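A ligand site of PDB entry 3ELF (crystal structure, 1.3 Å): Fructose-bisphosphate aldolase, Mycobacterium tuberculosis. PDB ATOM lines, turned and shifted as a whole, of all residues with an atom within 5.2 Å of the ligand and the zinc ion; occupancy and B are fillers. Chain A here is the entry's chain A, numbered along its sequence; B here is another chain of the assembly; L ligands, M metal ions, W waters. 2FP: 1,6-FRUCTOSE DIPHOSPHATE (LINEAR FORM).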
ATOM      1  N   ASN A  27     -31.138 -16.842 -26.744  1.00  0.00           N
ATOM      2  CA  ASN A  27     -31.052 -15.677 -25.885  1.00  0.00           C
ATOM      3  C   ASN A  27     -30.401 -14.513 -26.617  1.00  0.00           C
ATOM      4  O   ASN A  27     -29.342 -14.657 -27.241  1.00  0.00           O
ATOM      5  CB  ASN A  27     -30.272 -15.971 -24.615  1.00  0.00           C
ATOM      6  CG  ASN A  27     -31.059 -16.791 -23.633  1.00  0.00           C
ATOM      7  OD1 ASN A  27     -31.126 -18.017 -23.742  1.00  0.00           O
ATOM      8  ND2 ASN A  27     -31.680 -16.127 -22.654  1.00  0.00           N
ATOM      9  N   GLN A  51     -35.450 -15.066 -27.053  1.00  0.00           N
ATOM     10  CA  GLN A  51     -35.755 -14.916 -25.634  1.00  0.00           C
ATOM     11  C   GLN A  51     -34.852 -13.934 -24.903  1.00  0.00           C
ATOM     12  O   GLN A  51     -33.667 -13.798 -25.244  1.00  0.00           O
ATOM     13  CB  GLN A  51     -35.842 -16.258 -24.904  1.00  0.00           C
ATOM     14  CG  GLN A  51     -34.599 -17.124 -24.932  1.00  0.00           C
ATOM     15  CD  GLN A  51     -34.828 -18.471 -24.260  1.00  0.00           C
ATOM     16  OE1 GLN A  51     -35.938 -19.014 -24.293  1.00  0.00           O
ATOM     17  NE2 GLN A  51     -33.776 -19.014 -23.650  1.00  0.00           N
ATOM     18  N   SER A  53     -33.551 -13.030 -21.055  1.00  0.00           N
ATOM     19  CA  SER A  53     -33.445 -13.309 -19.632  1.00  0.00           C
ATOM     20  C   SER A  53     -33.646 -12.021 -18.836  1.00  0.00           C
ATOM     21  O   SER A  53     -33.681 -10.933 -19.398  1.00  0.00           O
ATOM     22  CB  SER A  53     -32.067 -13.890 -19.335  1.00  0.00           C
ATOM     23  OG  SER A  53     -31.085 -12.915 -19.581  1.00  0.00           O
ATOM     24  N   GLY A  55     -31.458 -10.703 -16.853  1.00  0.00           N
ATOM     25  CA  GLY A  55     -30.205  -9.960 -17.048  1.00  0.00           C
ATOM     26  C   GLY A  55     -30.078  -9.398 -18.453  1.00  0.00           C
ATOM     27  O   GLY A  55     -29.533  -8.309 -18.651  1.00  0.00           O
ATOM     28  N   GLY A  56     -30.547 -10.137 -19.445  1.00  0.00           N
ATOM     29  CA  GLY A  56     -30.533  -9.652 -20.818  1.00  0.00           C
ATOM     30  C   GLY A  56     -31.423  -8.432 -20.974  1.00  0.00           C
ATOM     31  O   GLY A  56     -31.048  -7.461 -21.635  1.00  0.00           O
ATOM     32  N   ASP A  95     -37.182 -15.476 -20.396  1.00  0.00           N
ATOM     33  CA  ASP A  95     -36.514 -16.617 -19.770  1.00  0.00           C
ATOM     34  C   ASP A  95     -36.611 -16.521 -18.231  1.00  0.00           C
ATOM     35  O   ASP A  95     -37.249 -15.602 -17.688  1.00  0.00           O
ATOM     36  CB  ASP A  95     -35.062 -16.643 -20.260  1.00  0.00           C
ATOM     37  CG  ASP A  95     -34.425 -18.026 -20.181  1.00  0.00           C
ATOM     38  OD1 ASP A  95     -35.077 -19.013 -19.797  1.00  0.00           O
ATOM     39  OD2 ASP A  95     -33.215 -18.081 -20.525  1.00  0.00           O
ATOM     40  N   HIS A  96     -35.996 -17.486 -17.534  1.00  0.00           N
ATOM     41  CA  HIS A  96     -36.073 -17.661 -16.070  1.00  0.00           C
ATOM     42  C   HIS A  96     -36.532 -16.455 -15.250  1.00  0.00           C
ATOM     43  O   HIS A  96     -35.789 -15.488 -15.089  1.00  0.00           O
ATOM     44  CB  HIS A  96     -34.714 -18.092 -15.490  1.00  0.00           C
ATOM     45  CG  HIS A  96     -34.168 -19.358 -16.076  1.00  0.00           C
ATOM     46  ND1 HIS A  96     -34.447 -20.605 -15.565  1.00  0.00           N
ATOM     47  CD2 HIS A  96     -33.328 -19.558 -17.124  1.00  0.00           C
ATOM     48  CE1 HIS A  96     -33.809 -21.518 -16.279  1.00  0.00           C
ATOM     49  NE2 HIS A  96     -33.118 -20.913 -17.220  1.00  0.00           N
ATOM     50  N   VAL A 211     -27.250 -28.921 -18.229  1.00  0.00           N
ATOM     51  CA  VAL A 211     -26.445 -27.925 -17.533  1.00  0.00           C
ATOM     52  C   VAL A 211     -26.290 -26.668 -18.391  1.00  0.00           C
ATOM     53  O   VAL A 211     -25.935 -26.776 -19.575  1.00  0.00           O
ATOM     54  CB  VAL A 211     -25.024 -28.488 -17.174  1.00  0.00           C
ATOM     55  CG1 VAL A 211     -24.164 -27.433 -16.473  1.00  0.00           C
ATOM     56  CG2 VAL A 211     -25.127 -29.738 -16.303  1.00  0.00           C
ATOM     57  N   HIS A 212     -26.528 -25.497 -17.810  1.00  0.00           N
ATOM     58  CA  HIS A 212     -26.245 -24.225 -18.480  1.00  0.00           C
ATOM     59  C   HIS A 212     -24.734 -24.053 -18.592  1.00  0.00           C
ATOM     60  O   HIS A 212     -24.017 -24.290 -17.615  1.00  0.00           O
ATOM     61  CB  HIS A 212     -26.784 -23.052 -17.656  1.00  0.00           C
ATOM     62  CG  HIS A 212     -28.282 -22.968 -17.599  1.00  0.00           C
ATOM     63  ND1 HIS A 212     -28.968 -22.955 -16.415  1.00  0.00           N
ATOM     64  CD2 HIS A 212     -29.211 -22.844 -18.580  1.00  0.00           C
ATOM     65  CE1 HIS A 212     -30.267 -22.838 -16.656  1.00  0.00           C
ATOM     66  NE2 HIS A 212     -30.439 -22.762 -17.967  1.00  0.00           N
ATOM     67  N   GLY A 213     -24.277 -23.610 -19.760  1.00  0.00           N
ATOM     68  CA  GLY A 213     -22.851 -23.392 -19.986  1.00  0.00           C
ATOM     69  C   GLY A 213     -22.257 -24.410 -20.934  1.00  0.00           C
ATOM     70  O   GLY A 213     -22.937 -25.342 -21.371  1.00  0.00           O
ATOM     71  N   VAL A 214     -20.980 -24.225 -21.249  1.00  0.00           N
ATOM     72  CA  VAL A 214     -20.262 -25.110 -22.168  1.00  0.00           C
ATOM     73  C   VAL A 214     -19.004 -25.643 -21.506  1.00  0.00           C
ATOM     74  O   VAL A 214     -18.124 -24.870 -21.121  1.00  0.00           O
ATOM     75  CB  VAL A 214     -19.917 -24.397 -23.496  1.00  0.00           C
ATOM     76  CG1 VAL A 214     -18.944 -25.233 -24.340  1.00  0.00           C
ATOM     77  CG2 VAL A 214     -21.181 -24.127 -24.274  1.00  0.00           C
ATOM     78  N   PHE A 251     -35.685 -27.868 -23.363  1.00  0.00           N
ATOM     79  CA  PHE A 251     -34.330 -28.339 -23.085  1.00  0.00           C
ATOM     80  C   PHE A 251     -33.467 -27.107 -22.792  1.00  0.00           C
ATOM     81  O   PHE A 251     -33.008 -26.435 -23.724  1.00  0.00           O
ATOM     82  CB  PHE A 251     -33.867 -29.110 -24.327  1.00  0.00           C
ATOM     83  CG  PHE A 251     -32.476 -29.728 -24.250  1.00  0.00           C
ATOM     84  CD1 PHE A 251     -31.536 -29.391 -23.289  1.00  0.00           C
ATOM     85  CD2 PHE A 251     -32.113 -30.647 -25.240  1.00  0.00           C
ATOM     86  CE1 PHE A 251     -30.251 -29.959 -23.308  1.00  0.00           C
ATOM     87  CE2 PHE A 251     -30.850 -31.221 -25.260  1.00  0.00           C
ATOM     88  CZ  PHE A 251     -29.921 -30.881 -24.289  1.00  0.00           C
ATOM     89  N   HIS A 252     -33.301 -26.788 -21.514  1.00  0.00           N
ATOM     90  CA  HIS A 252     -32.383 -25.728 -21.100  1.00  0.00           C
ATOM     91  C   HIS A 252     -30.946 -26.229 -21.159  1.00  0.00           C
ATOM     92  O   HIS A 252     -30.687 -27.409 -20.978  1.00  0.00           O
ATOM     93  CB  HIS A 252     -32.694 -25.267 -19.686  1.00  0.00           C
ATOM     94  CG  HIS A 252     -33.877 -24.355 -19.595  1.00  0.00           C
ATOM     95  ND1 HIS A 252     -33.753 -23.017 -19.271  1.00  0.00           N
ATOM     96  CD2 HIS A 252     -35.187 -24.576 -19.823  1.00  0.00           C
ATOM     97  CE1 HIS A 252     -34.945 -22.459 -19.297  1.00  0.00           C
ATOM     98  NE2 HIS A 252     -35.841 -23.373 -19.636  1.00  0.00           N
ATOM     99  N   GLY A 253     -30.011 -25.316 -21.369  1.00  0.00           N
ATOM    100  CA  GLY A 253     -28.611 -25.706 -21.388  1.00  0.00           C
ATOM    101  C   GLY A 253     -28.204 -26.421 -22.662  1.00  0.00           C
ATOM    102  O   GLY A 253     -27.324 -27.284 -22.639  1.00  0.00           O
ATOM    103  N   GLY A 254     -28.796 -26.044 -23.789  1.00  0.00           N
ATOM    104  CA  GLY A 254     -28.546 -26.721 -25.061  1.00  0.00           C
ATOM    105  C   GLY A 254     -27.129 -26.604 -25.600  1.00  0.00           C
ATOM    106  O   GLY A 254     -26.655 -27.509 -26.282  1.00  0.00           O
ATOM    107  N   SER A 255     -26.433 -25.506 -25.308  1.00  0.00           N
ATOM    108  CA  SER A 255     -25.089 -25.309 -25.850  1.00  0.00           C
ATOM    109  C   SER A 255     -24.156 -26.424 -25.429  1.00  0.00           C
ATOM    110  O   SER A 255     -24.228 -26.898 -24.290  1.00  0.00           O
ATOM    111  CB  SER A 255     -24.498 -23.975 -25.399  1.00  0.00           C
ATOM    112  OG  SER A 255     -25.257 -22.879 -25.871  1.00  0.00           O
ATOM    113  N   ASN A 274     -33.113 -24.276 -25.641  1.00  0.00           N
ATOM    114  CA  ASN A 274     -32.535 -22.985 -25.352  1.00  0.00           C
ATOM    115  C   ASN A 274     -31.042 -23.008 -25.629  1.00  0.00           C
ATOM    116  O   ASN A 274     -30.341 -23.933 -25.217  1.00  0.00           O
ATOM    117  CB  ASN A 274     -32.715 -22.610 -23.882  1.00  0.00           C
ATOM    118  CG  ASN A 274     -34.163 -22.375 -23.458  1.00  0.00           C
ATOM    119  OD1 ASN A 274     -34.419 -21.919 -22.342  1.00  0.00           O
ATOM    120  ND2 ASN A 274     -35.115 -22.661 -24.339  1.00  0.00           N
ATOM    121  N   VAL A 275     -30.567 -21.968 -26.323  1.00  0.00           N
ATOM    122  CA  VAL A 275     -29.159 -21.804 -26.651  1.00  0.00           C
ATOM    123  C   VAL A 275     -28.756 -20.370 -26.279  1.00  0.00           C
ATOM    124  O   VAL A 275     -29.425 -19.391 -26.668  1.00  0.00           O
ATOM    125  CB  VAL A 275     -28.910 -22.071 -28.155  1.00  0.00           C
ATOM    126  CG1 VAL A 275     -27.483 -21.714 -28.558  1.00  0.00           C
ATOM    127  CG2 VAL A 275     -29.189 -23.537 -28.490  1.00  0.00           C
ATOM    128  N   ASP A 276     -27.680 -20.234 -25.515  1.00  0.00           N
ATOM    129  CA  ASP A 276     -27.106 -18.921 -25.236  1.00  0.00           C
ATOM    130  C   ASP A 276     -25.597 -18.973 -25.362  1.00  0.00           C
ATOM    131  O   ASP A 276     -25.017 -18.243 -26.157  1.00  0.00           O
ATOM    132  CB  ASP A 276     -27.521 -18.424 -23.837  1.00  0.00           C
ATOM    133  CG  ASP A 276     -27.297 -16.920 -23.644  1.00  0.00           C
ATOM    134  OD1 ASP A 276     -26.795 -16.239 -24.564  1.00  0.00           O
ATOM    135  OD2 ASP A 276     -27.673 -16.413 -22.553  1.00  0.00           O
ATOM    136  N   THR A 277     -24.953 -19.845 -24.602  1.00  0.00           N
ATOM    137  CA  THR A 277     -23.499 -19.829 -24.530  1.00  0.00           C
ATOM    138  C   THR A 277     -22.832 -20.006 -25.908  1.00  0.00           C
ATOM    139  O   THR A 277     -21.885 -19.278 -26.241  1.00  0.00           O
ATOM    140  CB  THR A 277     -23.002 -20.869 -23.510  1.00  0.00           C
ATOM    141  OG1 THR A 277     -23.602 -20.612 -22.237  1.00  0.00           O
ATOM    142  CG2 THR A 277     -21.506 -20.785 -23.344  1.00  0.00           C
ATOM    143  N   ASP A 278     -23.318 -20.943 -26.715  1.00  0.00           N
ATOM    144  CA  ASP A 278     -22.711 -21.180 -28.018  1.00  0.00           C
ATOM    145  C   ASP A 278     -22.901 -20.010 -28.987  1.00  0.00           C
ATOM    146  O   ASP A 278     -22.019 -19.734 -29.794  1.00  0.00           O
ATOM    147  CB  ASP A 278     -23.213 -22.479 -28.633  1.00  0.00           C
ATOM    148  CG  ASP A 278     -22.446 -23.710 -28.154  1.00  0.00           C
ATOM    149  OD1 ASP A 278     -21.407 -23.574 -27.471  1.00  0.00           O
ATOM    150  OD2 ASP A 278     -22.911 -24.833 -28.462  1.00  0.00           O
ATOM    151  N   LYS B 308     -16.891 -18.476 -20.554  1.00  0.00           N
ATOM    152  CA  LYS B 308     -18.174 -17.845 -20.874  1.00  0.00           C
ATOM    153  C   LYS B 308     -18.316 -16.451 -20.293  1.00  0.00           C
ATOM    154  O   LYS B 308     -18.835 -15.551 -20.966  1.00  0.00           O
ATOM    155  CB  LYS B 308     -19.320 -18.726 -20.395  1.00  0.00           C
ATOM    156  CG  LYS B 308     -20.705 -18.079 -20.460  1.00  0.00           C
ATOM    157  CD  LYS B 308     -21.741 -18.973 -19.785  1.00  0.00           C
ATOM    158  CE  LYS B 308     -23.091 -18.269 -19.667  1.00  0.00           C
ATOM    159  NZ  LYS B 308     -23.721 -18.092 -21.001  1.00  0.00           N
ATOM    160  N   ASP B 312     -19.340 -13.762 -23.093  1.00  0.00           N
ATOM    161  CA  ASP B 312     -20.674 -13.173 -23.006  1.00  0.00           C
ATOM    162  C   ASP B 312     -20.573 -11.729 -23.533  1.00  0.00           C
ATOM    163  O   ASP B 312     -19.812 -10.943 -22.983  1.00  0.00           O
ATOM    164  CB  ASP B 312     -21.102 -13.180 -21.538  1.00  0.00           C
ATOM    165  CG  ASP B 312     -22.508 -12.641 -21.306  1.00  0.00           C
ATOM    166  OD1 ASP B 312     -23.138 -13.118 -20.339  1.00  0.00           O
ATOM    167  OD2 ASP B 312     -22.974 -11.752 -22.046  1.00  0.00           O
ATOM    168  N   ARG B 314     -22.241  -9.121 -23.214  1.00  0.00           N
ATOM    169  CA  ARG B 314     -22.514  -8.090 -22.218  1.00  0.00           C
ATOM    170  C   ARG B 314     -21.283  -7.694 -21.429  1.00  0.00           C
ATOM    171  O   ARG B 314     -21.185  -6.560 -20.970  1.00  0.00           O
ATOM    172  CB  ARG B 314     -23.636  -8.518 -21.278  1.00  0.00           C
ATOM    173  CG  ARG B 314     -24.942  -8.744 -21.997  1.00  0.00           C
ATOM    174  CD  ARG B 314     -25.945  -9.406 -21.085  1.00  0.00           C
ATOM    175  NE  ARG B 314     -25.566 -10.794 -20.820  1.00  0.00           N
ATOM    176  CZ  ARG B 314     -26.317 -11.663 -20.169  1.00  0.00           C
ATOM    177  NH1 ARG B 314     -27.488 -11.293 -19.677  1.00  0.00           N
ATOM    178  NH2 ARG B 314     -25.877 -12.908 -19.988  1.00  0.00           N
HETATM  179  P6  2FP L   1     -28.417 -14.992 -18.380  1.00  0.00           P
HETATM  180  O6  2FP L   1     -29.004 -16.125 -19.367  1.00  0.00           O
HETATM  181  C6  2FP L   1     -29.181 -17.485 -18.963  1.00  0.00           C
HETATM  182  C5  2FP L   1     -29.731 -18.259 -20.162  1.00  0.00           C
HETATM  183  O5  2FP L   1     -28.724 -18.273 -21.177  1.00  0.00           O
HETATM  184  C4  2FP L   1     -30.030 -19.719 -19.887  1.00  0.00           C
HETATM  185  O4  2FP L   1     -30.660 -19.918 -18.604  1.00  0.00           O
HETATM  186  C3  2FP L   1     -30.904 -20.283 -20.999  1.00  0.00           C
HETATM  187  O3  2FP L   1     -32.243 -20.470 -20.487  1.00  0.00           O
HETATM  188  C2  2FP L   1     -30.340 -21.610 -21.434  1.00  0.00           C
HETATM  189  O2  2FP L   1     -30.923 -22.613 -21.066  1.00  0.00           O
HETATM  190  C1  2FP L   1     -29.091 -21.708 -22.318  1.00  0.00           C
HETATM  191  O1  2FP L   1     -28.062 -22.623 -21.827  1.00  0.00           O
HETATM  192  O61 2FP L   1     -29.179 -15.180 -17.084  1.00  0.00           O
HETATM  193  O62 2FP L   1     -26.932 -15.263 -18.281  1.00  0.00           O
HETATM  194  O63 2FP L   1     -28.728 -13.719 -19.113  1.00  0.00           O
HETATM  195  P1  2FP L   1     -26.633 -22.758 -22.591  1.00  0.00           P
HETATM  196  O11 2FP L   1     -25.941 -21.455 -22.245  1.00  0.00           O
HETATM  197  O12 2FP L   1     -27.037 -22.776 -24.046  1.00  0.00           O
HETATM  198  O13 2FP L   1     -25.971 -24.046 -22.138  1.00  0.00           O
HETATM  199 ZN    ZN M   1     -32.072 -21.823 -18.822  1.00  0.00          ZN
HETATM  200  O   HOH W   1     -25.713 -16.152 -20.544  1.00  0.00           O
HETATM  201  O   HOH W   2     -28.740 -19.849 -16.731  1.00  0.00           O
HETATM  202  O   HOH W   3     -28.715 -13.810 -22.000  1.00  0.00           O
HETATM  203  O   HOH W   4     -31.603 -16.441 -16.625  1.00  0.00           O
HETATM  204  O   HOH W   5     -26.438 -19.719 -20.375  1.00  0.00           O
HETATM  205  O   HOH W   6     -28.399 -16.362 -14.820  1.00  0.00           O
HETATM  206  O   HOH W   7     -30.375 -13.127 -15.959  1.00  0.00           O
HETATM  207  O   HOH W   8     -25.544 -17.047 -16.876  1.00  0.00           O
HETATM  208  O   HOH W   9     -25.696 -13.492 -16.483  1.00  0.00           O
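Asn 27 touches the ligand (OD1 to O5, 3.5 Å). Gln 51 touches the ligand. Val 211 touches the ligand (O to O13, 3.7 Å). Gly 254 touches the ligand. CA of Val 275 touches O12 of the ligand, at 3.5 Å. Hydrophobic or aromatic side chains within 4 Å of the ligand: His 96, His 212 and His 252. Of the 24 residues printed, 17 come within 4 Å of the ligand.
Water W5 bridges an oxygen (O11) of the ligand (2.6 Å) and the side-chain amino group (NZ) of Lys 308 of chain B (3.2 Å). Water W7 lies within hydrogen-bond range of O61 of the ligand and N of Gly 55. Water W1 lies within hydrogen-bond range of an oxygen (O62) of the ligand (2.7 Å), the side-chain amino group (NZ) of Lys 308 of chain B (2.8 Å), the side-chain carboxylate (OD2) of Asp 276 (2.8 Å) and the guanidinium group (NH2) of Arg 314 of chain B (3.3 Å). Water W3 lies within hydrogen-bond range of the side-chain carboxylate (OD2) of Asp 276 (2.9 Å) and an oxygen (O63) of the ligand (2.9 Å).
The side-chain amide nitrogen of Gln 51 sits at hydrogen-bond distance from the side-chain carboxylate of Asp 95 (3.3 Å). The side-chain hydroxyl (OG) of Ser 255 lies within hydrogen-bond range of the backbone NH (N) of Asp 278, at 2.9 Å. The backbone carbonyl oxygen (O) of Val 275 sits at hydrogen-bond distance from the backbone NH (N) of Asn 27, 3.1 Å away. OG of Ser 53 is in hydrogen-bond range of N of Gly 56 (2.8 Å). The side-chain carboxylate of Asp 312 of chain B lies within salt-bridge range of the guanidinium group of Arg 314 of chain B, 2.8 Å away. The side-chain hydroxyl (OG) of Ser 255 is in hydrogen-bond range of the backbone NH (N) of Thr 277, 3.3 Å away. The side-chain amide nitrogen of Gln 51 lies within hydrogen-bond range of the side-chain amide oxygen of Asn 274 (3.3 Å). NE2 of Gln 51 sits at hydrogen-bond distance from OD1 of Asn 27 (2.8 Å).
Within 4 Å of the zinc ion: His 96, His 212 and His 252. The nearest printed residue that does not touch the zinc ion is Asp 95 (4.2 Å).
The zinc ion is bound by NE2 of His 212 (2.1 Å). The zinc ion is bound by ND1 of His 252 (2.1 Å). The zinc ion is bound by a ring nitrogen (NE2) of His 96, 2.1 Å away. The zinc ion is bound by an oxygen (O3) of the ligand. O4 of the ligand is bound to the zinc ion (2.4 Å). The zinc ion has five donor atoms within binding distance. Slightly farther from the zinc ion lies O2 of the ligand (2.6 Å).
O11 of the ligand sits at hydrogen-bond distance from OG1 of Thr 277, 2.5 Å away. OD2 of Asp 95 lies close to O3 of the ligand (2.6 Å). N of Asp 276 is in hydrogen-bond range of O12 of the ligand, 3.0 Å away. An oxygen (O12) of the ligand is in hydrogen-bond range of the backbone NH (N) of Ser 255. An oxygen (O12) of the ligand is in hydrogen-bond range of the side-chain hydroxyl (OG) of Ser 255 (2.6 Å). OG of Ser 53 lies within hydrogen-bond range of O63 of the ligand (2.5 Å). O11 of the ligand lies within hydrogen-bond range of N of Thr 277, 3.0 Å away. NH1 of Arg 314 of chain B is in salt-bridge range of O63 of the ligand, 2.8 Å away. OD2 of Asp 276 is in hydrogen-bond range of O5 of the ligand (2.5 Å). The backbone NH of Gly 253 lies within hydrogen-bond range of an oxygen (O2) of the ligand. N of Gly 213 lies within hydrogen-bond range of O13 of the ligand, at 3.0 Å. The side-chain amide oxygen (OD1) of Asn 274 sits close to an oxygen (O3) of the ligand (3.2 Å).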
